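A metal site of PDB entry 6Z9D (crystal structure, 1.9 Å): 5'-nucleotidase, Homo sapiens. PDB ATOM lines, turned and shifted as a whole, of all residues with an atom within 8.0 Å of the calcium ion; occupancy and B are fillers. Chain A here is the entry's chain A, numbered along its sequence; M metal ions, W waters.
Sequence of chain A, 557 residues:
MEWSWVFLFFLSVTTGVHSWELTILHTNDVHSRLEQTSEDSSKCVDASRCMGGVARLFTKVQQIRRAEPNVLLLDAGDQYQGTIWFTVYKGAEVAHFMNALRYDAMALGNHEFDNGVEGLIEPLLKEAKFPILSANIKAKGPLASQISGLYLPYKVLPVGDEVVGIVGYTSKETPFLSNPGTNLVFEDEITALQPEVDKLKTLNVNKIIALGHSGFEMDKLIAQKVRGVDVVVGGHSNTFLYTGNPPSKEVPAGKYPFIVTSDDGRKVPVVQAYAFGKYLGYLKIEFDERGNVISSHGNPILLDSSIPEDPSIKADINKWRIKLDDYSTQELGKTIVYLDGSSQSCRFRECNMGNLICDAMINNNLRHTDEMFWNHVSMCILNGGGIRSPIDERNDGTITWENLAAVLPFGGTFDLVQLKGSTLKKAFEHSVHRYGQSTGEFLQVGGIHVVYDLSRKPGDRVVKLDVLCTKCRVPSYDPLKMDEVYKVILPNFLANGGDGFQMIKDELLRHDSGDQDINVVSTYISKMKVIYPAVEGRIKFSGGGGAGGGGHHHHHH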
ATOM      1  N   LYS A 201      19.314  18.494 -38.110  1.00  0.00           N
ATOM      2  CA  LYS A 201      20.237  17.352 -38.091  1.00  0.00           C
ATOM      3  C   LYS A 201      21.171  17.381 -39.311  1.00  0.00           C
ATOM      4  O   LYS A 201      22.318  16.940 -39.211  1.00  0.00           O
ATOM      5  CB  LYS A 201      19.461  16.023 -38.116  1.00  0.00           C
ATOM      6  CG  LYS A 201      18.738  15.716 -36.808  1.00  0.00           C
ATOM      7  CD  LYS A 201      19.573  14.796 -35.921  1.00  0.00           C
ATOM      8  CE  LYS A 201      19.469  15.147 -34.460  1.00  0.00           C
ATOM      9  NZ  LYS A 201      20.137  16.440 -34.155  1.00  0.00           N
ATOM     10  N   VAL A 205      23.263  20.281 -36.387  1.00  0.00           N
ATOM     11  CA  VAL A 205      22.851  20.819 -35.077  1.00  0.00           C
ATOM     12  C   VAL A 205      22.456  19.565 -34.308  1.00  0.00           C
ATOM     13  O   VAL A 205      21.507  18.912 -34.692  1.00  0.00           O
ATOM     14  CB  VAL A 205      21.718  21.858 -35.167  1.00  0.00           C
ATOM     15  CG1 VAL A 205      21.252  22.268 -33.781  1.00  0.00           C
ATOM     16  CG2 VAL A 205      22.167  23.085 -35.953  1.00  0.00           C
ATOM     17  N   ASN A 206      23.257  19.168 -33.312  1.00  0.00           N
ATOM     18  CA  ASN A 206      22.984  17.941 -32.571  1.00  0.00           C
ATOM     19  C   ASN A 206      22.306  18.173 -31.205  1.00  0.00           C
ATOM     20  O   ASN A 206      22.040  17.194 -30.502  1.00  0.00           O
ATOM     21  CB  ASN A 206      24.272  17.088 -32.439  1.00  0.00           C
ATOM     22  CG  ASN A 206      25.428  17.730 -31.713  1.00  0.00           C
ATOM     23  OD1 ASN A 206      25.276  18.611 -30.867  1.00  0.00           O
ATOM     24  ND2 ASN A 206      26.635  17.298 -32.044  1.00  0.00           N
ATOM     25  N   LYS A 207      22.025  19.430 -30.821  1.00  0.00           N
ATOM     26  CA  LYS A 207      21.329  19.750 -29.565  1.00  0.00           C
ATOM     27  C   LYS A 207      20.058  20.499 -29.939  1.00  0.00           C
ATOM     28  O   LYS A 207      20.147  21.576 -30.543  1.00  0.00           O
ATOM     29  CB  LYS A 207      22.211  20.500 -28.566  1.00  0.00           C
ATOM     30  CG  LYS A 207      23.357  19.641 -28.027  1.00  0.00           C
ATOM     31  CD  LYS A 207      24.413  20.449 -27.248  1.00  0.00           C
ATOM     32  CE  LYS A 207      25.397  21.242 -28.093  1.00  0.00           C
ATOM     33  NZ  LYS A 207      26.222  20.373 -28.977  1.00  0.00           N
ATOM     34  N   ILE A 208      18.858  19.877 -29.696  1.00  0.00           N
ATOM     35  CA  ILE A 208      17.601  20.449 -30.176  1.00  0.00           C
ATOM     36  C   ILE A 208      16.539  20.525 -29.080  1.00  0.00           C
ATOM     37  O   ILE A 208      16.194  19.500 -28.461  1.00  0.00           O
ATOM     38  CB  ILE A 208      17.108  19.692 -31.459  1.00  0.00           C
ATOM     39  CG1 ILE A 208      18.114  19.875 -32.624  1.00  0.00           C
ATOM     40  CG2 ILE A 208      15.701  20.159 -31.904  1.00  0.00           C
ATOM     41  CD1 ILE A 208      17.803  19.008 -33.867  1.00  0.00           C
ATOM     42  N   ILE A 209      16.018  21.736 -28.870  1.00  0.00           N
ATOM     43  CA  ILE A 209      14.943  22.008 -27.907  1.00  0.00           C
ATOM     44  C   ILE A 209      13.647  22.261 -28.682  1.00  0.00           C
ATOM     45  O   ILE A 209      13.676  23.046 -29.620  1.00  0.00           O
ATOM     46  CB  ILE A 209      15.285  23.233 -27.001  1.00  0.00           C
ATOM     47  CG1 ILE A 209      16.696  23.098 -26.334  1.00  0.00           C
ATOM     48  CG2 ILE A 209      14.185  23.487 -25.952  1.00  0.00           C
ATOM     49  CD1 ILE A 209      17.159  24.417 -25.569  1.00  0.00           C
ATOM     50  N   GLY A 228      14.878  13.312 -32.775  1.00  0.00           N
ATOM     51  CA  GLY A 228      15.905  14.354 -32.696  1.00  0.00           C
ATOM     52  C   GLY A 228      15.665  15.404 -31.620  1.00  0.00           C
ATOM     53  O   GLY A 228      16.544  16.212 -31.333  1.00  0.00           O
ATOM     54  N   VAL A 229      14.456  15.441 -31.066  1.00  0.00           N
ATOM     55  CA  VAL A 229      14.133  16.423 -30.016  1.00  0.00           C
ATOM     56  C   VAL A 229      14.759  15.968 -28.713  1.00  0.00           C
ATOM     57  O   VAL A 229      14.496  14.865 -28.256  1.00  0.00           O
ATOM     58  CB  VAL A 229      12.611  16.669 -29.902  1.00  0.00           C
ATOM     59  CG1 VAL A 229      12.253  17.469 -28.650  1.00  0.00           C
ATOM     60  CG2 VAL A 229      12.082  17.374 -31.171  1.00  0.00           C
ATOM     61  N   ASP A 230      15.643  16.792 -28.151  1.00  0.00           N
ATOM     62  CA  ASP A 230      16.341  16.446 -26.896  1.00  0.00           C
ATOM     63  C   ASP A 230      15.549  16.788 -25.618  1.00  0.00           C
ATOM     64  O   ASP A 230      15.653  16.083 -24.609  1.00  0.00           O
ATOM     65  CB  ASP A 230      17.724  17.089 -26.877  1.00  0.00           C
ATOM     66  CG  ASP A 230      18.622  16.522 -27.959  1.00  0.00           C
ATOM     67  OD1 ASP A 230      18.699  15.285 -28.086  1.00  0.00           O
ATOM     68  OD2 ASP A 230      19.237  17.318 -28.698  1.00  0.00           O
ATOM     69  N   VAL A 231      14.829  17.914 -25.635  1.00  0.00           N
ATOM     70  CA  VAL A 231      14.075  18.447 -24.497  1.00  0.00           C
ATOM     71  C   VAL A 231      12.840  19.110 -25.037  1.00  0.00           C
ATOM     72  O   VAL A 231      12.887  19.726 -26.103  1.00  0.00           O
ATOM     73  CB  VAL A 231      14.905  19.509 -23.692  1.00  0.00           C
ATOM     74  CG1 VAL A 231      14.200  19.896 -22.397  1.00  0.00           C
ATOM     75  CG2 VAL A 231      16.309  19.013 -23.394  1.00  0.00           C
ATOM     76  N   ARG A 266      15.261   7.115 -26.572  1.00  0.00           N
ATOM     77  CA  ARG A 266      15.936   8.138 -25.770  1.00  0.00           C
ATOM     78  C   ARG A 266      15.089   8.611 -24.602  1.00  0.00           C
ATOM     79  O   ARG A 266      13.857   8.557 -24.673  1.00  0.00           O
ATOM     80  CB  ARG A 266      16.306   9.353 -26.622  1.00  0.00           C
ATOM     81  CG  ARG A 266      17.427   9.114 -27.616  1.00  0.00           C
ATOM     82  CD  ARG A 266      17.475  10.230 -28.648  1.00  0.00           C
ATOM     83  NE  ARG A 266      16.231  10.268 -29.410  1.00  0.00           N
ATOM     84  CZ  ARG A 266      15.328  11.232 -29.311  1.00  0.00           C
ATOM     85  NH1 ARG A 266      14.199  11.177 -30.021  1.00  0.00           N
ATOM     86  NH2 ARG A 266      15.535  12.272 -28.508  1.00  0.00           N
ATOM     87  N   PHE A 287      24.984  17.168 -21.841  1.00  0.00           N
ATOM     88  CA  PHE A 287      25.105  16.599 -23.179  1.00  0.00           C
ATOM     89  C   PHE A 287      26.510  16.059 -23.369  1.00  0.00           C
ATOM     90  O   PHE A 287      27.468  16.585 -22.794  1.00  0.00           O
ATOM     91  CB  PHE A 287      24.874  17.670 -24.253  1.00  0.00           C
ATOM     92  CG  PHE A 287      23.476  18.186 -24.395  1.00  0.00           C
ATOM     93  CD1 PHE A 287      22.521  17.486 -25.137  1.00  0.00           C
ATOM     94  CD2 PHE A 287      23.120  19.434 -23.886  1.00  0.00           C
ATOM     95  CE1 PHE A 287      21.237  17.995 -25.342  1.00  0.00           C
ATOM     96  CE2 PHE A 287      21.818  19.945 -24.085  1.00  0.00           C
ATOM     97  CZ  PHE A 287      20.893  19.207 -24.791  1.00  0.00           C
ATOM     98  N   ASP A 288      26.663  15.060 -24.258  1.00  0.00           N
ATOM     99  CA  ASP A 288      28.007  14.642 -24.630  1.00  0.00           C
ATOM    100  C   ASP A 288      28.321  15.441 -25.912  1.00  0.00           C
ATOM    101  O   ASP A 288      27.459  16.184 -26.395  1.00  0.00           O
ATOM    102  CB  ASP A 288      28.110  13.122 -24.825  1.00  0.00           C
ATOM    103  CG  ASP A 288      27.321  12.508 -25.969  1.00  0.00           C
ATOM    104  OD1 ASP A 288      26.869  13.265 -26.864  1.00  0.00           O
ATOM    105  OD2 ASP A 288      27.160  11.284 -25.988  1.00  0.00           O
ATOM    106  N   ARG A 290      28.303  14.643 -28.922  1.00  0.00           N
ATOM    107  CA  ARG A 290      27.409  14.294 -30.033  1.00  0.00           C
ATOM    108  C   ARG A 290      25.957  14.726 -29.846  1.00  0.00           C
ATOM    109  O   ARG A 290      25.097  14.335 -30.643  1.00  0.00           O
ATOM    110  CB  ARG A 290      27.492  12.793 -30.318  1.00  0.00           C
ATOM    111  CG  ARG A 290      28.819  12.365 -30.941  1.00  0.00           C
ATOM    112  CD  ARG A 290      29.029  12.966 -32.324  1.00  0.00           C
ATOM    113  NE  ARG A 290      30.065  12.226 -33.021  1.00  0.00           N
ATOM    114  CZ  ARG A 290      29.835  11.331 -33.970  1.00  0.00           C
ATOM    115  NH1 ARG A 290      28.595  11.109 -34.396  1.00  0.00           N
ATOM    116  NH2 ARG A 290      30.848  10.682 -34.528  1.00  0.00           N
ATOM    117  N   GLY A 291      25.692  15.520 -28.810  1.00  0.00           N
ATOM    118  CA  GLY A 291      24.337  16.002 -28.493  1.00  0.00           C
ATOM    119  C   GLY A 291      23.417  15.001 -27.812  1.00  0.00           C
ATOM    120  O   GLY A 291      22.208  15.240 -27.718  1.00  0.00           O
ATOM    121  N   ASN A 292      23.944  13.857 -27.345  1.00  0.00           N
ATOM    122  CA  ASN A 292      23.117  12.883 -26.627  1.00  0.00           C
ATOM    123  C   ASN A 292      22.917  13.430 -25.203  1.00  0.00           C
ATOM    124  O   ASN A 292      23.862  13.985 -24.647  1.00  0.00           O
ATOM    125  CB  ASN A 292      23.840  11.525 -26.522  1.00  0.00           C
ATOM    126  CG  ASN A 292      24.221  10.860 -27.818  1.00  0.00           C
ATOM    127  OD1 ASN A 292      25.409  10.703 -28.149  1.00  0.00           O
ATOM    128  ND2 ASN A 292      23.243  10.414 -28.566  1.00  0.00           N
ATOM    129  N   VAL A 293      21.739  13.237 -24.605  1.00  0.00           N
ATOM    130  CA  VAL A 293      21.486  13.699 -23.239  1.00  0.00           C
ATOM    131  C   VAL A 293      21.900  12.587 -22.294  1.00  0.00           C
ATOM    132  O   VAL A 293      21.318  11.493 -22.340  1.00  0.00           O
ATOM    133  CB  VAL A 293      20.016  14.134 -23.046  1.00  0.00           C
ATOM    134  CG1 VAL A 293      19.690  14.374 -21.566  1.00  0.00           C
ATOM    135  CG2 VAL A 293      19.672  15.345 -23.888  1.00  0.00           C
HETATM  136 CA    CA M   1      20.846  15.458 -29.644  1.00  0.00          CA
HETATM  137  O   HOH W   1      18.657  13.200 -30.742  1.00  0.00           O
HETATM  138  O   HOH W   2      19.191  15.805 -31.389  1.00  0.00           O
HETATM  139  O   HOH W   3      21.879  13.090 -30.496  1.00  0.00           O
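Water W2 lies within hydrogen-bond range of the backbone carbonyl oxygen (O) of Gly 228 and the side-chain amino group (NZ) of Lys 201.
The calcium ion is bound by O of Asn 206 (2.3 Å), O of Gly 291 (2.4 Å), water W2 (2.4 Å), OD2 of Asp 230 (2.6 Å), OD1 of Asp 230 (2.7 Å) and water W3 (2.7 Å). The calcium ion has six donor atoms within binding distance.
Of the 17 residues printed, 3 come within 4 Å of the calcium ion. The nearest printed residue that does not touch the calcium ion is Asn 292 (4.2 Å).
The side-chain amino group of Lys 207 sits at hydrogen-bond distance from the side-chain amide oxygen of Asn 206 (2.8 Å). N of Gly 291 is in hydrogen-bond range of OD1 of Asp 288 (3.2 Å). The backbone NH (N) of Asp 230 lies within hydrogen-bond range of the backbone carbonyl oxygen (O) of Ile 208 (2.8 Å).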
